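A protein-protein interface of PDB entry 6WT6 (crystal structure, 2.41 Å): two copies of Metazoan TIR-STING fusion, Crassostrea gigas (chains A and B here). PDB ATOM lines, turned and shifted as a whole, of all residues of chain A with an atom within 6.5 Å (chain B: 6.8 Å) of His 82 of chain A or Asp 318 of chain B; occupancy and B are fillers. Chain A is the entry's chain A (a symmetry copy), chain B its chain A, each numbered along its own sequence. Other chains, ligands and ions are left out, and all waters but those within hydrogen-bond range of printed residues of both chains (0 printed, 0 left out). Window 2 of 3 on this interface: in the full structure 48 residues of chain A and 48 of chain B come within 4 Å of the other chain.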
ATOM      1  N   ARG A  26     -16.572  35.788  27.660  1.00  0.00           N
ATOM      2  CA  ARG A  26     -17.873  35.233  27.300  1.00  0.00           C
ATOM      3  C   ARG A  26     -17.938  33.732  27.570  1.00  0.00           C
ATOM      4  O   ARG A  26     -17.133  33.196  28.335  1.00  0.00           O
ATOM      5  CB  ARG A  26     -18.172  35.528  25.827  1.00  0.00           C
ATOM      6  CG  ARG A  26     -19.651  35.644  25.464  1.00  0.00           C
ATOM      7  CD  ARG A  26     -19.820  35.849  23.965  1.00  0.00           C
ATOM      8  NE  ARG A  26     -18.920  34.988  23.200  1.00  0.00           N
ATOM      9  CZ  ARG A  26     -18.785  35.027  21.877  1.00  0.00           C
ATOM     10  NH1 ARG A  26     -19.494  35.887  21.158  1.00  0.00           N
ATOM     11  NH2 ARG A  26     -17.938  34.206  21.271  1.00  0.00           N
ATOM     12  N   HIS A  27     -18.895  33.043  26.936  1.00  0.00           N
ATOM     13  CA  HIS A  27     -19.058  31.610  27.181  1.00  0.00           C
ATOM     14  C   HIS A  27     -17.891  30.794  26.634  1.00  0.00           C
ATOM     15  O   HIS A  27     -17.273  30.046  27.405  1.00  0.00           O
ATOM     16  CB  HIS A  27     -20.405  31.140  26.631  1.00  0.00           C
ATOM     17  CG  HIS A  27     -20.408  29.720  26.156  1.00  0.00           C
ATOM     18  ND1 HIS A  27     -19.999  28.667  26.948  1.00  0.00           N
ATOM     19  CD2 HIS A  27     -20.783  29.178  24.974  1.00  0.00           C
ATOM     20  CE1 HIS A  27     -20.116  27.539  26.268  1.00  0.00           C
ATOM     21  NE2 HIS A  27     -20.592  27.822  25.069  1.00  0.00           N
ATOM     22  N   PRO A  28     -17.548  30.869  25.340  1.00  0.00           N
ATOM     23  CA  PRO A  28     -16.441  30.029  24.858  1.00  0.00           C
ATOM     24  C   PRO A  28     -15.081  30.524  25.315  1.00  0.00           C
ATOM     25  O   PRO A  28     -14.157  29.714  25.460  1.00  0.00           O
ATOM     26  CB  PRO A  28     -16.593  30.104  23.334  1.00  0.00           C
ATOM     27  CG  PRO A  28     -17.173  31.444  23.100  1.00  0.00           C
ATOM     28  CD  PRO A  28     -18.093  31.715  24.262  1.00  0.00           C
ATOM     29  N   HIS A  29     -14.938  31.821  25.573  1.00  0.00           N
ATOM     30  CA  HIS A  29     -13.629  32.390  25.857  1.00  0.00           C
ATOM     31  C   HIS A  29     -13.171  32.052  27.272  1.00  0.00           C
ATOM     32  O   HIS A  29     -13.926  32.201  28.239  1.00  0.00           O
ATOM     33  CB  HIS A  29     -13.659  33.905  25.662  1.00  0.00           C
ATOM     34  CG  HIS A  29     -14.020  34.330  24.273  1.00  0.00           C
ATOM     35  ND1 HIS A  29     -14.563  35.567  23.995  1.00  0.00           N
ATOM     36  CD2 HIS A  29     -13.917  33.688  23.084  1.00  0.00           C
ATOM     37  CE1 HIS A  29     -14.779  35.668  22.695  1.00  0.00           C
ATOM     38  NE2 HIS A  29     -14.396  34.542  22.120  1.00  0.00           N
ATOM     39  N   VAL A  30     -11.924  31.593  27.385  1.00  0.00           N
ATOM     40  CA  VAL A  30     -11.280  31.360  28.673  1.00  0.00           C
ATOM     41  C   VAL A  30      -9.921  32.052  28.674  1.00  0.00           C
ATOM     42  O   VAL A  30      -9.239  32.106  29.703  1.00  0.00           O
ATOM     43  CB  VAL A  30     -11.138  29.857  28.979  1.00  0.00           C
ATOM     44  CG1 VAL A  30     -12.501  29.175  28.990  1.00  0.00           C
ATOM     45  CG2 VAL A  30     -10.217  29.192  27.979  1.00  0.00           C
ATOM     46  N   VAL A  77      -4.710  23.416  18.877  1.00  0.00           N
ATOM     47  CA  VAL A  77      -4.495  24.822  18.549  1.00  0.00           C
ATOM     48  C   VAL A  77      -5.826  25.510  18.271  1.00  0.00           C
ATOM     49  O   VAL A  77      -6.124  26.574  18.824  1.00  0.00           O
ATOM     50  CB  VAL A  77      -3.529  24.951  17.358  1.00  0.00           C
ATOM     51  CG1 VAL A  77      -3.512  26.378  16.828  1.00  0.00           C
ATOM     52  CG2 VAL A  77      -2.127  24.520  17.768  1.00  0.00           C
ATOM     53  N   VAL A  78      -6.653  24.899  17.421  1.00  0.00           N
ATOM     54  CA  VAL A  78      -7.933  25.506  17.078  1.00  0.00           C
ATOM     55  C   VAL A  78      -8.862  25.526  18.287  1.00  0.00           C
ATOM     56  O   VAL A  78      -9.642  26.472  18.462  1.00  0.00           O
ATOM     57  CB  VAL A  78      -8.550  24.777  15.869  1.00  0.00           C
ATOM     58  CG1 VAL A  78      -9.985  25.216  15.643  1.00  0.00           C
ATOM     59  CG2 VAL A  78      -7.715  25.063  14.633  1.00  0.00           C
ATOM     60  N   ASP A  79      -8.788  24.506  19.148  1.00  0.00           N
ATOM     61  CA  ASP A  79      -9.502  24.570  20.421  1.00  0.00           C
ATOM     62  C   ASP A  79      -9.058  25.780  21.239  1.00  0.00           C
ATOM     63  O   ASP A  79      -9.877  26.421  21.907  1.00  0.00           O
ATOM     64  CB  ASP A  79      -9.297  23.279  21.217  1.00  0.00           C
ATOM     65  CG  ASP A  79     -10.136  22.123  20.693  1.00  0.00           C
ATOM     66  OD1 ASP A  79     -10.967  22.346  19.790  1.00  0.00           O
ATOM     67  OD2 ASP A  79      -9.962  20.986  21.185  1.00  0.00           O
ATOM     68  N   ALA A  80      -7.766  26.115  21.186  1.00  0.00           N
ATOM     69  CA  ALA A  80      -7.282  27.294  21.896  1.00  0.00           C
ATOM     70  C   ALA A  80      -7.742  28.577  21.216  1.00  0.00           C
ATOM     71  O   ALA A  80      -8.113  29.544  21.891  1.00  0.00           O
ATOM     72  CB  ALA A  80      -5.758  27.261  22.004  1.00  0.00           C
ATOM     73  N   ILE A  81      -7.721  28.607  19.882  1.00  0.00           N
ATOM     74  CA  ILE A  81      -8.192  29.782  19.153  1.00  0.00           C
ATOM     75  C   ILE A  81      -9.677  30.011  19.413  1.00  0.00           C
ATOM     76  O   ILE A  81     -10.128  31.154  19.571  1.00  0.00           O
ATOM     77  CB  ILE A  81      -7.893  29.629  17.649  1.00  0.00           C
ATOM     78  CG1 ILE A  81      -6.381  29.577  17.410  1.00  0.00           C
ATOM     79  CG2 ILE A  81      -8.530  30.758  16.855  1.00  0.00           C
ATOM     80  CD1 ILE A  81      -5.996  29.302  15.971  1.00  0.00           C
ATOM     81  N   HIS A  82     -10.461  28.929  19.473  1.00  0.00           N
ATOM     82  CA  HIS A  82     -11.892  29.062  19.731  1.00  0.00           C
ATOM     83  C   HIS A  82     -12.160  29.701  21.089  1.00  0.00           C
ATOM     84  O   HIS A  82     -13.126  30.460  21.238  1.00  0.00           O
ATOM     85  CB  HIS A  82     -12.569  27.693  19.644  1.00  0.00           C
ATOM     86  CG  HIS A  82     -14.052  27.739  19.850  1.00  0.00           C
ATOM     87  ND1 HIS A  82     -14.861  28.661  19.221  1.00  0.00           N
ATOM     88  CD2 HIS A  82     -14.873  26.978  20.613  1.00  0.00           C
ATOM     89  CE1 HIS A  82     -16.115  28.466  19.587  1.00  0.00           C
ATOM     90  NE2 HIS A  82     -16.150  27.449  20.430  1.00  0.00           N
ATOM     91  N   CYS A  83     -11.317  29.416  22.078  1.00  0.00           N
ATOM     92  CA  CYS A  83     -11.480  29.935  23.428  1.00  0.00           C
ATOM     93  C   CYS A  83     -10.722  31.231  23.665  1.00  0.00           C
ATOM     94  O   CYS A  83     -10.695  31.716  24.799  1.00  0.00           O
ATOM     95  CB  CYS A  83     -11.022  28.891  24.448  1.00  0.00           C
ATOM     96  SG  CYS A  83     -11.864  27.300  24.309  1.00  0.00           S
ATOM     97  N   SER A  84     -10.099  31.799  22.641  1.00  0.00           N
ATOM     98  CA  SER A  84      -9.350  33.038  22.786  1.00  0.00           C
ATOM     99  C   SER A  84     -10.121  34.180  22.140  1.00  0.00           C
ATOM    100  O   SER A  84     -10.498  34.103  20.964  1.00  0.00           O
ATOM    101  CB  SER A  84      -7.954  32.921  22.174  1.00  0.00           C
ATOM    102  OG  SER A  84      -7.111  32.125  22.990  1.00  0.00           O
ATOM    103  N   LYS A  85     -10.359  35.231  22.922  1.00  0.00           N
ATOM    104  CA  LYS A  85     -11.031  36.418  22.408  1.00  0.00           C
ATOM    105  C   LYS A  85     -10.252  37.027  21.247  1.00  0.00           C
ATOM    106  O   LYS A  85     -10.811  37.277  20.172  1.00  0.00           O
ATOM    107  CB  LYS A  85     -11.211  37.420  23.548  1.00  0.00           C
ATOM    108  CG  LYS A  85     -11.618  38.814  23.140  1.00  0.00           C
ATOM    109  CD  LYS A  85     -11.191  39.788  24.225  1.00  0.00           C
ATOM    110  CE  LYS A  85     -11.790  41.157  24.025  1.00  0.00           C
ATOM    111  NZ  LYS A  85     -13.232  41.146  24.371  1.00  0.00           N
ATOM    112  N   LEU B 311     -13.278  25.189  13.045  1.00  0.00           N
ATOM    113  CA  LEU B 311     -13.429  26.371  13.883  1.00  0.00           C
ATOM    114  C   LEU B 311     -14.764  27.072  13.637  1.00  0.00           C
ATOM    115  O   LEU B 311     -15.421  27.520  14.584  1.00  0.00           O
ATOM    116  CB  LEU B 311     -12.261  27.320  13.626  1.00  0.00           C
ATOM    117  CG  LEU B 311     -12.243  28.689  14.297  1.00  0.00           C
ATOM    118  CD1 LEU B 311     -12.403  28.545  15.801  1.00  0.00           C
ATOM    119  CD2 LEU B 311     -10.942  29.400  13.954  1.00  0.00           C
ATOM    120  N   LEU B 313     -17.625  25.800  12.446  1.00  0.00           N
ATOM    121  CA  LEU B 313     -18.722  25.001  12.980  1.00  0.00           C
ATOM    122  C   LEU B 313     -18.829  25.159  14.492  1.00  0.00           C
ATOM    123  O   LEU B 313     -19.936  25.236  15.040  1.00  0.00           O
ATOM    124  CB  LEU B 313     -18.531  23.531  12.595  1.00  0.00           C
ATOM    125  CG  LEU B 313     -19.656  22.555  12.947  1.00  0.00           C
ATOM    126  CD1 LEU B 313     -20.978  22.963  12.292  1.00  0.00           C
ATOM    127  CD2 LEU B 313     -19.281  21.132  12.551  1.00  0.00           C
ATOM    128  N   LYS B 314     -17.691  25.233  15.184  1.00  0.00           N
ATOM    129  CA  LYS B 314     -17.734  25.354  16.638  1.00  0.00           C
ATOM    130  C   LYS B 314     -18.199  26.737  17.082  1.00  0.00           C
ATOM    131  O   LYS B 314     -18.823  26.863  18.141  1.00  0.00           O
ATOM    132  CB  LYS B 314     -16.366  25.022  17.231  1.00  0.00           C
ATOM    133  CG  LYS B 314     -15.991  23.562  17.065  1.00  0.00           C
ATOM    134  CD  LYS B 314     -14.524  23.312  17.376  1.00  0.00           C
ATOM    135  CE  LYS B 314     -14.299  23.079  18.858  1.00  0.00           C
ATOM    136  NZ  LYS B 314     -13.809  24.294  19.549  1.00  0.00           N
ATOM    137  N   ARG B 315     -17.913  27.779  16.297  1.00  0.00           N
ATOM    138  CA  ARG B 315     -18.430  29.102  16.626  1.00  0.00           C
ATOM    139  C   ARG B 315     -19.948  29.138  16.509  1.00  0.00           C
ATOM    140  O   ARG B 315     -20.631  29.734  17.351  1.00  0.00           O
ATOM    141  CB  ARG B 315     -17.811  30.162  15.713  1.00  0.00           C
ATOM    142  CG  ARG B 315     -16.298  30.245  15.756  1.00  0.00           C
ATOM    143  CD  ARG B 315     -15.845  31.684  15.896  1.00  0.00           C
ATOM    144  NE  ARG B 315     -14.436  31.860  15.561  1.00  0.00           N
ATOM    145  CZ  ARG B 315     -14.005  32.370  14.413  1.00  0.00           C
ATOM    146  NH1 ARG B 315     -14.878  32.757  13.492  1.00  0.00           N
ATOM    147  NH2 ARG B 315     -12.705  32.502  14.187  1.00  0.00           N
ATOM    148  N   ILE B 316     -20.493  28.502  15.471  1.00  0.00           N
ATOM    149  CA  ILE B 316     -21.937  28.506  15.262  1.00  0.00           C
ATOM    150  C   ILE B 316     -22.636  27.697  16.347  1.00  0.00           C
ATOM    151  O   ILE B 316     -23.634  28.140  16.926  1.00  0.00           O
ATOM    152  CB  ILE B 316     -22.268  27.972  13.858  1.00  0.00           C
ATOM    153  CG1 ILE B 316     -21.629  28.858  12.788  1.00  0.00           C
ATOM    154  CG2 ILE B 316     -23.771  27.877  13.662  1.00  0.00           C
ATOM    155  CD1 ILE B 316     -21.684  28.256  11.411  1.00  0.00           C
ATOM    156  N   LEU B 317     -22.121  26.499  16.638  1.00  0.00           N
ATOM    157  CA  LEU B 317     -22.766  25.635  17.623  1.00  0.00           C
ATOM    158  C   LEU B 317     -22.740  26.257  19.014  1.00  0.00           C
ATOM    159  O   LEU B 317     -23.753  26.240  19.725  1.00  0.00           O
ATOM    160  CB  LEU B 317     -22.100  24.256  17.635  1.00  0.00           C
ATOM    161  CG  LEU B 317     -22.265  23.388  16.380  1.00  0.00           C
ATOM    162  CD1 LEU B 317     -21.402  22.135  16.459  1.00  0.00           C
ATOM    163  CD2 LEU B 317     -23.722  23.011  16.148  1.00  0.00           C
ATOM    164  N   ASP B 318     -21.597  26.819  19.422  1.00  0.00           N
ATOM    165  CA  ASP B 318     -21.512  27.424  20.748  1.00  0.00           C
ATOM    166  C   ASP B 318     -22.273  28.740  20.839  1.00  0.00           C
ATOM    167  O   ASP B 318     -22.599  29.178  21.945  1.00  0.00           O
ATOM    168  CB  ASP B 318     -20.053  27.635  21.148  1.00  0.00           C
ATOM    169  CG  ASP B 318     -19.359  26.340  21.497  1.00  0.00           C
ATOM    170  OD1 ASP B 318     -20.066  25.356  21.804  1.00  0.00           O
ATOM    171  OD2 ASP B 318     -18.112  26.298  21.467  1.00  0.00           O
ATOM    172  N   THR B 319     -22.559  29.376  19.704  1.00  0.00           N
ATOM    173  CA  THR B 319     -23.412  30.559  19.704  1.00  0.00           C
ATOM    174  C   THR B 319     -24.870  30.196  19.963  1.00  0.00           C
ATOM    175  O   THR B 319     -25.604  30.973  20.582  1.00  0.00           O
ATOM    176  CB  THR B 319     -23.257  31.297  18.368  1.00  0.00           C
ATOM    177  OG1 THR B 319     -22.059  32.084  18.394  1.00  0.00           O
ATOM    178  CG2 THR B 319     -24.456  32.199  18.073  1.00  0.00           C
ATOM    179  N   ASP B 320     -25.293  29.011  19.522  1.00  0.00           N
ATOM    180  CA  ASP B 320     -26.682  28.591  19.629  1.00  0.00           C
ATOM    181  C   ASP B 320     -26.881  27.845  20.944  1.00  0.00           C
ATOM    182  O   ASP B 320     -26.328  26.749  21.108  1.00  0.00           O
ATOM    183  CB  ASP B 320     -27.055  27.711  18.444  1.00  0.00           C
ATOM    184  CG  ASP B 320     -28.524  27.370  18.398  1.00  0.00           C
ATOM    185  OD1 ASP B 320     -29.244  27.651  19.378  1.00  0.00           O
ATOM    186  OD2 ASP B 320     -28.963  26.818  17.368  1.00  0.00           O
ATOM    187  N   PRO B 321     -27.657  28.380  21.890  1.00  0.00           N
ATOM    188  CA  PRO B 321     -27.739  27.743  23.216  1.00  0.00           C
ATOM    189  C   PRO B 321     -28.415  26.381  23.214  1.00  0.00           C
ATOM    190  O   PRO B 321     -28.116  25.560  24.090  1.00  0.00           O
ATOM    191  CB  PRO B 321     -28.530  28.765  24.047  1.00  0.00           C
ATOM    192  CG  PRO B 321     -28.343  30.071  23.320  1.00  0.00           C
ATOM    193  CD  PRO B 321     -28.315  29.698  21.869  1.00  0.00           C
ATOM    194  N   CYS B 323     -28.040  24.164  20.824  1.00  0.00           N
ATOM    195  CA  CYS B 323     -27.185  23.230  20.099  1.00  0.00           C
ATOM    196  C   CYS B 323     -25.831  23.001  20.751  1.00  0.00           C
ATOM    197  O   CYS B 323     -25.258  21.923  20.576  1.00  0.00           O
ATOM    198  CB  CYS B 323     -26.950  23.704  18.655  1.00  0.00           C
ATOM    199  SG  CYS B 323     -28.323  23.395  17.523  1.00  0.00           S
ATOM    200  N   SER B 324     -25.297  23.976  21.481  1.00  0.00           N
ATOM    201  CA  SER B 324     -24.031  23.764  22.165  1.00  0.00           C
ATOM    202  C   SER B 324     -24.203  22.735  23.276  1.00  0.00           C
ATOM    203  O   SER B 324     -25.282  22.590  23.858  1.00  0.00           O
ATOM    204  CB  SER B 324     -23.499  25.077  22.733  1.00  0.00           C
ATOM    205  OG  SER B 324     -24.391  25.617  23.684  1.00  0.00           O
ATOM    206  N   LYS B 325     -23.127  22.002  23.552  1.00  0.00           N
ATOM    207  CA  LYS B 325     -23.110  20.890  24.496  1.00  0.00           C
ATOM    208  C   LYS B 325     -24.047  19.756  24.089  1.00  0.00           C
ATOM    209  O   LYS B 325     -24.357  18.889  24.914  1.00  0.00           O
ATOM    210  CB  LYS B 325     -23.443  21.353  25.924  1.00  0.00           C
ATOM    211  CG  LYS B 325     -22.499  22.405  26.488  1.00  0.00           C
ATOM    212  CD  LYS B 325     -22.922  22.834  27.891  1.00  0.00           C
ATOM    213  CE  LYS B 325     -24.332  23.432  27.900  1.00  0.00           C
ATOM    214  NZ  LYS B 325     -24.722  23.959  29.245  1.00  0.00           N
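Of chain B, only Leu 311 (3.9 Å), Lys 314 (3.1 Å), Arg 315 (3.8 Å) and Asp 318 (2.5 Å) come within 4 Å of His 82 of chain A. Asp 318 of chain B touches just these residues of chain A: His 27 and His 82. Of the printed residues of chain B, His 27 of chain A touches Asp 318. Of the printed residues of chain B, Asp 79 of chain A touches Lys 314 (3.5 Å). Of the printed residues of chain A, Arg 315 of chain B touches His 82. Of the printed residues of chain A, Leu 311 of chain B touches Val 78 (3.7 Å) and His 82 (3.9 Å). Of the printed residues of chain A, Lys 314 of chain B touches Asp 79 (3.5 Å) and His 82 (3.1 Å). The nearest printed residue of chain A that does not touch Leu 311 of chain B is Ile 81 of chain A (4.01 Å).
The backbone carbonyl oxygen of Asp 79 of chain A lies within hydrogen-bond range of the side-chain sulfur of Cys 83 of chain A (3.2 Å). O of Arg 315 of chain B is in hydrogen-bond range of OG1 of Thr 319 of chain B (2.9 Å).
Among the printed residues, merely in contact across the chains: His 82 of chain A with Lys 314 of chain B, His 27 of chain A with Asp 318 of chain B, Val 78 of chain A with Leu 311 of chain B, His 82 of chain A with Arg 315 of chain B and His 82 of chain A with Leu 311 of chain B.
No position is printed for both chains. Of the 7 pairs that touch across the chains among the printed residues, none has its exchanged pair printed and touching as well.
OD2 of Asp 318 of chain B sits at hydrogen-bond distance from NE2 of His 82 of chain A, at 2.5 Å. NZ of Lys 314 of chain B is in salt-bridge range of OD1 of Asp 79 of chain A, at 3.5 Å.
Of the 13 printed residues of chain B, 4 touch a printed residue of chain A. Hydrophobic or aromatic side chains of chain B that line the printed part of chain A: Leu 311. Of the 14 printed residues of chain A, 4 touch a printed residue of chain B. Printed residues of chain A that touch a printed residue of chain B: His 27, Val 78, Asp 79 and His 82. Hydrophobic or aromatic side chains of chain A within 4 Å of the printed part of chain B: His 27, Val 78 and His 82. Among the printed residues, Asp or Glu carboxylates within 4 Å of a Lys or Arg side-chain nitrogen of the other chain: Asp 79 of chain A with Lys 314 of chain B.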
